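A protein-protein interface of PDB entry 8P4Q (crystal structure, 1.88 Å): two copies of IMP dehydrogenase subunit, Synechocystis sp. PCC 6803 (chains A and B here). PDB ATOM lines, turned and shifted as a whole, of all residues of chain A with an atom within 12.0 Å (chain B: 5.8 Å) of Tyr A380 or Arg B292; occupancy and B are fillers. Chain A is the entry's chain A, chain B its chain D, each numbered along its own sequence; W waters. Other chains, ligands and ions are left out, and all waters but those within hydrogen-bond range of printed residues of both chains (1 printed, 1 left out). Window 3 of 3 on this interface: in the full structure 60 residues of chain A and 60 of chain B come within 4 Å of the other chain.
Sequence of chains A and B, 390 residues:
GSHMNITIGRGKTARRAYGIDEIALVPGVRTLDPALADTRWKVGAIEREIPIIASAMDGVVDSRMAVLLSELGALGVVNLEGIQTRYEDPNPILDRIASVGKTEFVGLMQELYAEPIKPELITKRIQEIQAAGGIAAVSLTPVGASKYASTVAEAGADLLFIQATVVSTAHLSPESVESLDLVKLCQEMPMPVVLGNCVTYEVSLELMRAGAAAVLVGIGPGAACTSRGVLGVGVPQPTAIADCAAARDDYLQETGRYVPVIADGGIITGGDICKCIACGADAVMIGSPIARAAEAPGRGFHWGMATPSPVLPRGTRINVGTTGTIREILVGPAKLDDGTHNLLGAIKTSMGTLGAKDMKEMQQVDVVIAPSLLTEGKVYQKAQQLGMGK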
ATOM      1  N   ASP A 337     -27.061   0.199  12.608  1.00  0.00           N
ATOM      2  CA  ASP A 337     -25.832  -0.571  12.512  1.00  0.00           C
ATOM      3  C   ASP A 337     -24.675   0.021  13.308  1.00  0.00           C
ATOM      4  O   ASP A 337     -23.562  -0.503  13.227  1.00  0.00           O
ATOM      5  CB  ASP A 337     -25.428  -0.706  11.037  1.00  0.00           C
ATOM      6  CG  ASP A 337     -25.057   0.637  10.395  1.00  0.00           C
ATOM      7  OD1 ASP A 337     -25.132   1.678  11.082  1.00  0.00           O
ATOM      8  OD2 ASP A 337     -24.657   0.662   9.213  1.00  0.00           O
ATOM      9  N   LEU A 374     -10.391   2.389  15.771  1.00  0.00           N
ATOM     10  CA  LEU A 374     -11.406   3.107  15.020  1.00  0.00           C
ATOM     11  C   LEU A 374     -11.030   3.316  13.561  1.00  0.00           C
ATOM     12  O   LEU A 374     -11.813   3.909  12.817  1.00  0.00           O
ATOM     13  CB  LEU A 374     -11.676   4.463  15.680  1.00  0.00           C
ATOM     14  CG  LEU A 374     -11.997   4.409  17.176  1.00  0.00           C
ATOM     15  CD1 LEU A 374     -12.156   5.806  17.763  1.00  0.00           C
ATOM     16  CD2 LEU A 374     -13.252   3.584  17.426  1.00  0.00           C
ATOM     17  N   THR A 375      -9.861   2.842  13.135  1.00  0.00           N
ATOM     18  CA  THR A 375      -9.397   3.032  11.768  1.00  0.00           C
ATOM     19  C   THR A 375      -9.175   1.739  11.002  1.00  0.00           C
ATOM     20  O   THR A 375      -9.407   1.717   9.790  1.00  0.00           O
ATOM     21  CB  THR A 375      -8.089   3.845  11.758  1.00  0.00           C
ATOM     22  OG1 THR A 375      -7.029   3.070  12.336  1.00  0.00           O
ATOM     23  CG2 THR A 375      -8.256   5.143  12.537  1.00  0.00           C
ATOM     24  N   GLU A 376      -8.731   0.673  11.665  1.00  0.00           N
ATOM     25  CA  GLU A 376      -8.416  -0.571  10.976  1.00  0.00           C
ATOM     26  C   GLU A 376      -9.587  -1.012  10.111  1.00  0.00           C
ATOM     27  O   GLU A 376     -10.677  -1.290  10.620  1.00  0.00           O
ATOM     28  CB  GLU A 376      -8.068  -1.663  11.992  1.00  0.00           C
ATOM     29  CG  GLU A 376      -6.583  -1.837  12.255  1.00  0.00           C
ATOM     30  CD  GLU A 376      -6.261  -3.095  13.058  1.00  0.00           C
ATOM     31  OE1 GLU A 376      -7.144  -3.637  13.762  1.00  0.00           O
ATOM     32  OE2 GLU A 376      -5.107  -3.545  12.983  1.00  0.00           O
ATOM     33  N   GLY A 377      -9.364  -1.032   8.799  1.00  0.00           N
ATOM     34  CA  GLY A 377     -10.330  -1.575   7.863  1.00  0.00           C
ATOM     35  C   GLY A 377     -11.560  -0.737   7.597  1.00  0.00           C
ATOM     36  O   GLY A 377     -12.434  -1.176   6.847  1.00  0.00           O
ATOM     37  N   LYS A 378     -11.649   0.475   8.139  1.00  0.00           N
ATOM     38  CA  LYS A 378     -12.891   1.232   8.097  1.00  0.00           C
ATOM     39  C   LYS A 378     -12.935   2.239   6.949  1.00  0.00           C
ATOM     40  O   LYS A 378     -13.750   3.167   6.977  1.00  0.00           O
ATOM     41  CB  LYS A 378     -13.102   1.938   9.438  1.00  0.00           C
ATOM     42  CG  LYS A 378     -13.157   0.987  10.644  1.00  0.00           C
ATOM     43  CD  LYS A 378     -14.343   0.036  10.541  1.00  0.00           C
ATOM     44  CE  LYS A 378     -14.301  -1.055  11.610  1.00  0.00           C
ATOM     45  NZ  LYS A 378     -13.313  -2.118  11.273  1.00  0.00           N
ATOM     46  N   VAL A 379     -12.118   2.045   5.915  1.00  0.00           N
ATOM     47  CA  VAL A 379     -12.063   3.021   4.831  1.00  0.00           C
ATOM     48  C   VAL A 379     -13.422   3.153   4.148  1.00  0.00           C
ATOM     49  O   VAL A 379     -13.881   4.266   3.863  1.00  0.00           O
ATOM     50  CB  VAL A 379     -10.955   2.647   3.829  1.00  0.00           C
ATOM     51  CG1 VAL A 379     -11.201   1.273   3.223  1.00  0.00           C
ATOM     52  CG2 VAL A 379     -10.851   3.710   2.734  1.00  0.00           C
ATOM     53  N   TYR A 380     -14.088   2.029   3.873  1.00  0.00           N
ATOM     54  CA  TYR A 380     -15.385   2.094   3.203  1.00  0.00           C
ATOM     55  C   TYR A 380     -16.429   2.757   4.094  1.00  0.00           C
ATOM     56  O   TYR A 380     -17.198   3.613   3.637  1.00  0.00           O
ATOM     57  CB  TYR A 380     -15.855   0.697   2.796  1.00  0.00           C
ATOM     58  CG  TYR A 380     -14.967   0.005   1.800  1.00  0.00           C
ATOM     59  CD1 TYR A 380     -15.042   0.307   0.445  1.00  0.00           C
ATOM     60  CD2 TYR A 380     -14.067  -0.965   2.211  1.00  0.00           C
ATOM     61  CE1 TYR A 380     -14.232  -0.333  -0.470  1.00  0.00           C
ATOM     62  CE2 TYR A 380     -13.255  -1.608   1.306  1.00  0.00           C
ATOM     63  CZ  TYR A 380     -13.340  -1.289  -0.031  1.00  0.00           C
ATOM     64  OH  TYR A 380     -12.534  -1.935  -0.939  1.00  0.00           O
ATOM     65  N   GLN A 381     -16.489   2.348   5.365  1.00  0.00           N
ATOM     66  CA  GLN A 381     -17.474   2.916   6.282  1.00  0.00           C
ATOM     67  C   GLN A 381     -17.305   4.424   6.398  1.00  0.00           C
ATOM     68  O   GLN A 381     -18.292   5.169   6.415  1.00  0.00           O
ATOM     69  CB  GLN A 381     -17.360   2.258   7.660  1.00  0.00           C
ATOM     70  CG  GLN A 381     -17.816   0.809   7.700  1.00  0.00           C
ATOM     71  CD  GLN A 381     -17.763   0.208   9.098  1.00  0.00           C
ATOM     72  OE1 GLN A 381     -18.033   0.882  10.099  1.00  0.00           O
ATOM     73  NE2 GLN A 381     -17.430  -1.074   9.170  1.00  0.00           N
ATOM     74  N   LYS A 382     -16.057   4.895   6.467  1.00  0.00           N
ATOM     75  CA  LYS A 382     -15.815   6.330   6.558  1.00  0.00           C
ATOM     76  C   LYS A 382     -16.280   7.043   5.295  1.00  0.00           C
ATOM     77  O   LYS A 382     -16.947   8.082   5.365  1.00  0.00           O
ATOM     78  CB  LYS A 382     -14.331   6.602   6.815  1.00  0.00           C
ATOM     79  N   ALA A 383     -15.930   6.499   4.126  1.00  0.00           N
ATOM     80  CA  ALA A 383     -16.251   7.165   2.866  1.00  0.00           C
ATOM     81  C   ALA A 383     -17.752   7.195   2.609  1.00  0.00           C
ATOM     82  O   ALA A 383     -18.273   8.167   2.047  1.00  0.00           O
ATOM     83  CB  ALA A 383     -15.530   6.478   1.705  1.00  0.00           C
ATOM     84  N   GLN A 384     -18.459   6.131   2.976  1.00  0.00           N
ATOM     85  CA  GLN A 384     -19.880   5.999   2.691  1.00  0.00           C
ATOM     86  C   GLN A 384     -20.762   6.383   3.871  1.00  0.00           C
ATOM     87  O   GLN A 384     -21.983   6.236   3.786  1.00  0.00           O
ATOM     88  CB  GLN A 384     -20.176   4.563   2.241  1.00  0.00           C
ATOM     89  CG  GLN A 384     -19.413   4.179   0.978  1.00  0.00           C
ATOM     90  CD  GLN A 384     -19.468   2.696   0.657  1.00  0.00           C
ATOM     91  OE1 GLN A 384     -20.438   2.007   0.971  1.00  0.00           O
ATOM     92  NE2 GLN A 384     -18.419   2.201   0.010  1.00  0.00           N
ATOM     93  N   GLN A 385     -20.175   6.870   4.964  1.00  0.00           N
ATOM     94  CA  GLN A 385     -20.931   7.312   6.136  1.00  0.00           C
ATOM     95  C   GLN A 385     -21.880   6.219   6.621  1.00  0.00           C
ATOM     96  O   GLN A 385     -23.081   6.423   6.786  1.00  0.00           O
ATOM     97  CB  GLN A 385     -21.680   8.609   5.828  1.00  0.00           C
ATOM     98  CG  GLN A 385     -20.740   9.768   5.466  1.00  0.00           C
ATOM     99  CD  GLN A 385     -21.446  11.101   5.327  1.00  0.00           C
ATOM    100  OE1 GLN A 385     -20.859  12.151   5.589  1.00  0.00           O
ATOM    101  NE2 GLN A 385     -22.692  11.073   4.873  1.00  0.00           N
ATOM    102  N   LEU A 386     -21.316   5.042   6.851  1.00  0.00           N
ATOM    103  CA  LEU A 386     -22.035   3.877   7.335  1.00  0.00           C
ATOM    104  C   LEU A 386     -21.358   3.345   8.586  1.00  0.00           C
ATOM    105  O   LEU A 386     -20.151   3.505   8.761  1.00  0.00           O
ATOM    106  CB  LEU A 386     -22.090   2.792   6.265  1.00  0.00           C
ATOM    107  CG  LEU A 386     -22.981   3.073   5.054  1.00  0.00           C
ATOM    108  CD1 LEU A 386     -22.751   2.020   3.970  1.00  0.00           C
ATOM    109  CD2 LEU A 386     -24.438   3.154   5.442  1.00  0.00           C
ATOM    110  N   GLY A 387     -22.148   2.698   9.441  1.00  0.00           N
ATOM    111  CA  GLY A 387     -21.627   2.075  10.641  1.00  0.00           C
ATOM    112  C   GLY A 387     -20.812   3.010  11.507  1.00  0.00           C
ATOM    113  O   GLY A 387     -21.311   4.047  11.949  1.00  0.00           O
ATOM    114  N   MET A 388     -19.549   2.654  11.737  1.00  0.00           N
ATOM    115  CA  MET A 388     -18.663   3.445  12.578  1.00  0.00           C
ATOM    116  C   MET A 388     -18.220   4.738  11.915  1.00  0.00           C
ATOM    117  O   MET A 388     -17.616   5.581  12.584  1.00  0.00           O
ATOM    118  CB  MET A 388     -17.441   2.603  12.956  1.00  0.00           C
ATOM    119  CG  MET A 388     -17.766   1.348  13.757  1.00  0.00           C
ATOM    120  SD  MET A 388     -16.340   0.296  14.116  1.00  0.00           S
ATOM    121  CE  MET A 388     -15.250   1.447  14.942  1.00  0.00           C
ATOM    122  N   GLY A 389     -18.512   4.921  10.635  1.00  0.00           N
ATOM    123  CA  GLY A 389     -18.124   6.116   9.922  1.00  0.00           C
ATOM    124  C   GLY A 389     -19.200   7.173   9.823  1.00  0.00           C
ATOM    125  O   GLY A 389     -19.043   8.122   9.042  1.00  0.00           O
ATOM    126  N   LYS A 390     -20.292   7.050  10.574  1.00  0.00           N
ATOM    127  CA  LYS A 390     -21.376   8.031  10.453  1.00  0.00           C
ATOM    128  C   LYS A 390     -21.071   9.285  11.279  1.00  0.00           C
ATOM    129  O   LYS A 390     -20.483   9.220  12.368  1.00  0.00           O
ATOM    130  CB  LYS A 390     -22.712   7.447  10.911  1.00  0.00           C
ATOM    131  CG  LYS A 390     -23.253   6.297  10.066  1.00  0.00           C
ATOM    132  CD  LYS A 390     -24.735   6.135  10.338  1.00  0.00           C
ATOM    133  CE  LYS A 390     -25.221   4.743   9.988  1.00  0.00           C
ATOM    134  NZ  LYS A 390     -26.491   4.458  10.732  1.00  0.00           N
ATOM    135  N   ALA B 223     -13.999  -4.786   7.360  1.00  0.00           N
ATOM    136  CA  ALA B 223     -14.468  -3.621   6.618  1.00  0.00           C
ATOM    137  C   ALA B 223     -15.961  -3.390   6.793  1.00  0.00           C
ATOM    138  O   ALA B 223     -16.424  -2.248   6.675  1.00  0.00           O
ATOM    139  CB  ALA B 223     -14.137  -3.779   5.133  1.00  0.00           C
ATOM    140  N   ILE B 268      -7.033  -5.016   3.106  1.00  0.00           N
ATOM    141  CA  ILE B 268      -7.462  -4.414   1.855  1.00  0.00           C
ATOM    142  C   ILE B 268      -6.484  -4.712   0.727  1.00  0.00           C
ATOM    143  O   ILE B 268      -6.899  -4.994  -0.399  1.00  0.00           O
ATOM    144  CB  ILE B 268      -7.648  -2.887   2.022  1.00  0.00           C
ATOM    145  CG1 ILE B 268      -8.645  -2.562   3.141  1.00  0.00           C
ATOM    146  CG2 ILE B 268      -8.071  -2.269   0.687  1.00  0.00           C
ATOM    147  CD1 ILE B 268     -10.052  -2.970   2.832  1.00  0.00           C
ATOM    148  N   GLY B 287     -12.436 -10.912   3.462  1.00  0.00           N
ATOM    149  CA  GLY B 287     -13.771 -10.850   2.907  1.00  0.00           C
ATOM    150  C   GLY B 287     -13.925  -9.777   1.851  1.00  0.00           C
ATOM    151  O   GLY B 287     -14.222 -10.081   0.694  1.00  0.00           O
ATOM    152  N   SER B 288     -13.717  -8.516   2.232  1.00  0.00           N
ATOM    153  CA  SER B 288     -13.979  -7.416   1.307  1.00  0.00           C
ATOM    154  C   SER B 288     -13.160  -7.501   0.025  1.00  0.00           C
ATOM    155  O   SER B 288     -13.719  -7.212  -1.050  1.00  0.00           O
ATOM    156  CB  SER B 288     -13.747  -6.079   2.028  1.00  0.00           C
ATOM    157  OG  SER B 288     -12.388  -5.680   2.010  1.00  0.00           O
ATOM    158  N   PRO B 289     -11.880  -7.883   0.042  1.00  0.00           N
ATOM    159  CA  PRO B 289     -11.140  -7.946  -1.234  1.00  0.00           C
ATOM    160  C   PRO B 289     -11.735  -8.940  -2.218  1.00  0.00           C
ATOM    161  O   PRO B 289     -11.598  -8.754  -3.434  1.00  0.00           O
ATOM    162  CB  PRO B 289      -9.716  -8.348  -0.808  1.00  0.00           C
ATOM    163  CG  PRO B 289      -9.636  -8.012   0.675  1.00  0.00           C
ATOM    164  CD  PRO B 289     -11.039  -8.238   1.199  1.00  0.00           C
ATOM    165  N   ILE B 290     -12.394  -9.987  -1.726  1.00  0.00           N
ATOM    166  CA  ILE B 290     -12.994 -10.982  -2.603  1.00  0.00           C
ATOM    167  C   ILE B 290     -14.437 -10.617  -2.952  1.00  0.00           C
ATOM    168  O   ILE B 290     -14.929 -11.006  -4.014  1.00  0.00           O
ATOM    169  CB  ILE B 290     -12.902 -12.370  -1.944  1.00  0.00           C
ATOM    170  CG1 ILE B 290     -11.431 -12.778  -1.825  1.00  0.00           C
ATOM    171  CG2 ILE B 290     -13.671 -13.388  -2.746  1.00  0.00           C
ATOM    172  CD1 ILE B 290     -11.180 -14.039  -1.016  1.00  0.00           C
ATOM    173  N   ALA B 291     -15.122  -9.863  -2.087  1.00  0.00           N
ATOM    174  CA  ALA B 291     -16.439  -9.340  -2.437  1.00  0.00           C
ATOM    175  C   ALA B 291     -16.372  -8.407  -3.637  1.00  0.00           C
ATOM    176  O   ALA B 291     -17.407  -8.118  -4.248  1.00  0.00           O
ATOM    177  CB  ALA B 291     -17.053  -8.620  -1.233  1.00  0.00           C
ATOM    178  N   ARG B 292     -15.180  -7.922  -3.982  1.00  0.00           N
ATOM    179  CA  ARG B 292     -15.004  -7.080  -5.157  1.00  0.00           C
ATOM    180  C   ARG B 292     -14.854  -7.886  -6.441  1.00  0.00           C
ATOM    181  O   ARG B 292     -14.669  -7.290  -7.509  1.00  0.00           O
ATOM    182  CB  ARG B 292     -13.788  -6.170  -4.971  1.00  0.00           C
ATOM    183  CG  ARG B 292     -13.881  -5.272  -3.743  1.00  0.00           C
ATOM    184  CD  ARG B 292     -12.631  -4.410  -3.592  1.00  0.00           C
ATOM    185  NE  ARG B 292     -12.873  -3.042  -4.029  1.00  0.00           N
ATOM    186  CZ  ARG B 292     -11.954  -2.085  -4.056  1.00  0.00           C
ATOM    187  NH1 ARG B 292     -10.705  -2.317  -3.685  1.00  0.00           N
ATOM    188  NH2 ARG B 292     -12.301  -0.863  -4.445  1.00  0.00           N
ATOM    189  N   ALA B 293     -14.927  -9.211  -6.364  1.00  0.00           N
ATOM    190  CA  ALA B 293     -14.825 -10.050  -7.545  1.00  0.00           C
ATOM    191  C   ALA B 293     -16.139 -10.048  -8.315  1.00  0.00           C
ATOM    192  O   ALA B 293     -17.224  -9.990  -7.731  1.00  0.00           O
ATOM    193  CB  ALA B 293     -14.455 -11.482  -7.160  1.00  0.00           C
ATOM    194  N   ALA B 294     -16.026 -10.138  -9.640  1.00  0.00           N
ATOM    195  CA  ALA B 294     -17.209 -10.207 -10.489  1.00  0.00           C
ATOM    196  C   ALA B 294     -18.101 -11.380 -10.119  1.00  0.00           C
ATOM    197  O   ALA B 294     -19.326 -11.298 -10.263  1.00  0.00           O
ATOM    198  CB  ALA B 294     -16.795 -10.298 -11.956  1.00  0.00           C
ATOM    199  N   ALA B 296     -18.525 -12.608  -7.087  1.00  0.00           N
ATOM    200  CA  ALA B 296     -18.952 -12.591  -5.696  1.00  0.00           C
ATOM    201  C   ALA B 296     -20.476 -12.490  -5.617  1.00  0.00           C
ATOM    202  O   ALA B 296     -21.087 -11.709  -6.357  1.00  0.00           O
ATOM    203  CB  ALA B 296     -18.317 -11.421  -4.951  1.00  0.00           C
ATOM    204  N   ILE B 318     -21.708  -2.351   3.099  1.00  0.00           N
ATOM    205  CA  ILE B 318     -20.926  -1.353   2.384  1.00  0.00           C
ATOM    206  C   ILE B 318     -20.926  -1.699   0.902  1.00  0.00           C
ATOM    207  O   ILE B 318     -21.158  -2.843   0.496  1.00  0.00           O
ATOM    208  CB  ILE B 318     -19.483  -1.241   2.924  1.00  0.00           C
ATOM    209  CG1 ILE B 318     -18.804  -2.613   2.893  1.00  0.00           C
ATOM    210  CG2 ILE B 318     -19.492  -0.637   4.313  1.00  0.00           C
ATOM    211  CD1 ILE B 318     -17.316  -2.567   3.166  1.00  0.00           C
ATOM    212  N   ASN B 319     -20.689  -0.680   0.082  1.00  0.00           N
ATOM    213  CA  ASN B 319     -20.565  -0.840  -1.364  1.00  0.00           C
ATOM    214  C   ASN B 319     -19.077  -0.908  -1.684  1.00  0.00           C
ATOM    215  O   ASN B 319     -18.379   0.109  -1.668  1.00  0.00           O
ATOM    216  CB  ASN B 319     -21.256   0.303  -2.097  1.00  0.00           C
ATOM    217  CG  ASN B 319     -21.253   0.108  -3.595  1.00  0.00           C
ATOM    218  OD1 ASN B 319     -20.503  -0.712  -4.121  1.00  0.00           O
ATOM    219  ND2 ASN B 319     -22.095   0.858  -4.293  1.00  0.00           N
ATOM    220  N   VAL B 320     -18.585  -2.114  -1.972  1.00  0.00           N
ATOM    221  CA  VAL B 320     -17.173  -2.271  -2.308  1.00  0.00           C
ATOM    222  C   VAL B 320     -16.940  -2.239  -3.805  1.00  0.00           C
ATOM    223  O   VAL B 320     -15.786  -2.101  -4.238  1.00  0.00           O
ATOM    224  CB  VAL B 320     -16.582  -3.575  -1.735  1.00  0.00           C
ATOM    225  CG1 VAL B 320     -16.652  -3.561  -0.213  1.00  0.00           C
ATOM    226  CG2 VAL B 320     -17.313  -4.784  -2.286  1.00  0.00           C
ATOM    227  N   GLY B 321     -17.994  -2.360  -4.608  1.00  0.00           N
ATOM    228  CA  GLY B 321     -17.861  -2.341  -6.043  1.00  0.00           C
ATOM    229  C   GLY B 321     -17.338  -3.657  -6.585  1.00  0.00           C
ATOM    230  O   GLY B 321     -17.207  -4.667  -5.885  1.00  0.00           O
ATOM    231  N   THR B 322     -17.043  -3.629  -7.880  1.00  0.00           N
ATOM    232  CA  THR B 322     -16.517  -4.780  -8.599  1.00  0.00           C
ATOM    233  C   THR B 322     -15.330  -4.303  -9.414  1.00  0.00           C
ATOM    234  O   THR B 322     -15.487  -3.482 -10.322  1.00  0.00           O
ATOM    235  CB  THR B 322     -17.585  -5.408  -9.500  1.00  0.00           C
ATOM    236  OG1 THR B 322     -18.741  -5.722  -8.714  1.00  0.00           O
ATOM    237  CG2 THR B 322     -17.057  -6.681 -10.141  1.00  0.00           C
ATOM    238  N   THR B 323     -14.141  -4.806  -9.087  1.00  0.00           N
ATOM    239  CA  THR B 323     -12.907  -4.323  -9.686  1.00  0.00           C
ATOM    240  C   THR B 323     -12.266  -5.327 -10.633  1.00  0.00           C
ATOM    241  O   THR B 323     -11.359  -4.951 -11.383  1.00  0.00           O
ATOM    242  CB  THR B 323     -11.898  -3.957  -8.589  1.00  0.00           C
ATOM    243  OG1 THR B 323     -11.578  -5.132  -7.829  1.00  0.00           O
ATOM    244  CG2 THR B 323     -12.467  -2.888  -7.664  1.00  0.00           C
ATOM    245  N   GLY B 324     -12.703  -6.578 -10.618  1.00  0.00           N
ATOM    246  CA  GLY B 324     -12.133  -7.584 -11.491  1.00  0.00           C
ATOM    247  C   GLY B 324     -12.682  -8.948 -11.140  1.00  0.00           C
ATOM    248  O   GLY B 324     -13.566  -9.092 -10.289  1.00  0.00           O
ATOM    249  N   THR B 325     -12.171  -9.948 -11.849  1.00  0.00           N
ATOM    250  CA  THR B 325     -12.520 -11.331 -11.570  1.00  0.00           C
ATOM    251  C   THR B 325     -11.745 -11.839 -10.359  1.00  0.00           C
ATOM    252  O   THR B 325     -10.717 -11.280  -9.965  1.00  0.00           O
ATOM    253  CB  THR B 325     -12.248 -12.215 -12.787  1.00  0.00           C
ATOM    254  OG1 THR B 325     -10.839 -12.284 -13.028  1.00  0.00           O
ATOM    255  CG2 THR B 325     -12.948 -11.648 -14.011  1.00  0.00           C
ATOM    256  N   ILE B 329      -7.991 -10.969  -8.980  1.00  0.00           N
ATOM    257  CA  ILE B 329      -7.767 -10.518  -7.610  1.00  0.00           C
ATOM    258  C   ILE B 329      -6.711 -11.374  -6.925  1.00  0.00           C
ATOM    259  O   ILE B 329      -5.844 -10.858  -6.210  1.00  0.00           O
ATOM    260  CB  ILE B 329      -9.100 -10.516  -6.835  1.00  0.00           C
ATOM    261  CG1 ILE B 329      -9.981  -9.365  -7.336  1.00  0.00           C
ATOM    262  CG2 ILE B 329      -8.852 -10.413  -5.349  1.00  0.00           C
ATOM    263  CD1 ILE B 329     -11.419  -9.425  -6.872  1.00  0.00           C
ATOM    264  N   ASP B 338      -3.150  -0.170  -6.920  1.00  0.00           N
ATOM    265  CA  ASP B 338      -3.342  -0.032  -5.482  1.00  0.00           C
ATOM    266  C   ASP B 338      -3.092  -1.319  -4.707  1.00  0.00           C
ATOM    267  O   ASP B 338      -3.363  -1.366  -3.502  1.00  0.00           O
ATOM    268  CB  ASP B 338      -4.757   0.479  -5.207  1.00  0.00           C
ATOM    269  CG  ASP B 338      -5.831  -0.453  -5.748  1.00  0.00           C
ATOM    270  OD1 ASP B 338      -5.489  -1.587  -6.156  1.00  0.00           O
ATOM    271  OD2 ASP B 338      -7.012  -0.038  -5.795  1.00  0.00           O
ATOM    272  N   THR B 340      -4.650  -4.191  -4.768  1.00  0.00           N
ATOM    273  CA  THR B 340      -5.815  -4.999  -4.428  1.00  0.00           C
ATOM    274  C   THR B 340      -6.034  -6.153  -5.396  1.00  0.00           C
ATOM    275  O   THR B 340      -6.942  -6.963  -5.174  1.00  0.00           O
ATOM    276  CB  THR B 340      -7.079  -4.133  -4.376  1.00  0.00           C
ATOM    277  OG1 THR B 340      -7.329  -3.563  -5.667  1.00  0.00           O
ATOM    278  CG2 THR B 340      -6.927  -3.018  -3.343  1.00  0.00           C
HETATM  279  O   HOH W   1     -11.510  -4.067  -0.138  1.00  0.00           O
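The guanidinium group of Arg B292 sits close to the side-chain hydroxyl of Tyr A380 (3.3 Å). NE2 of Gln A381 sits at hydrogen-bond distance from O of Ala B223. The side-chain amide nitrogen (NE2) of Gln A384 sits at hydrogen-bond distance from the backbone carbonyl oxygen (O) of Asn B319.
O of Gln A381 sits at hydrogen-bond distance from N of Leu A386 (3.1 Å). The side-chain amide oxygen (OE1) of Gln A381 lies within hydrogen-bond range of the backbone NH (N) of Met A388, 2.8 Å away. The backbone carbonyl oxygen (O) of Val B320 sits at hydrogen-bond distance from the guanidinium group (NE) of Arg B292 (3.1 Å). The backbone carbonyl oxygen of Arg B292 lies within hydrogen-bond range of the backbone NH of Thr B323 (3.0 Å). The backbone NH (N) of Gly B321 lies within hydrogen-bond range of the side-chain amide oxygen (OD1) of Asn B319 (3.0 Å).
CA of Ala B223 touches O of Gly A377, at 3.2 Å. Tyr A380 touches Ile B268. Ile B318 touches Tyr A380. Asn B319 touches Tyr A380 (O to CD1, 3.95 Å). Tyr A380 touches Val B320 (CE1 to CA, 3.97 Å). Gln A384 touches Ile B318 (OE1 to CA, 3.7 Å).
Of the printed residues of chain B, Gly A377 touches Ala B223. Of the printed residues of chain B, Gln A384 touches Ile B318 and Asn B319. Leu A386 touches none of the printed residues of chain B. Pro B289 touches none of the printed residues of chain A. No residue of chain A comes within 4 Å of Ala B291. Of chain A, only Tyr A380 (3.2 Å) comes within 4 Å of Arg B292. No residue of chain A comes within 4 Å of Ala B293. No residue of chain A comes within 4 Å of Ala B294. No residue of chain A comes within 4 Å of Ala B296. Of chain A, only Tyr A380 (3.6 Å) and Gln A384 (3.7 Å) come within 4 Å of Ile B318. Of the printed residues of chain A, Asn B319 touches Tyr A380 and Gln A384. Val B320 touches one residue of chain A. No residue of chain A comes within 4 Å of Gly B321. No residue of chain A comes within 4 Å of Thr B323. The nearest residue of chain B that does not touch Tyr A380 is Ala B223 (4.1 Å).
Hydrophobic or aromatic side chains of chain A within 4 Å of the printed part of chain B: Tyr A380. Among the printed residues, 9 pairs touch across the chains.
No position is printed for both chains.
Water W1 bridges the side-chain hydroxyl of Tyr A380 (2.5 Å) and the side-chain hydroxyl of Ser B288 (2.8 Å).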
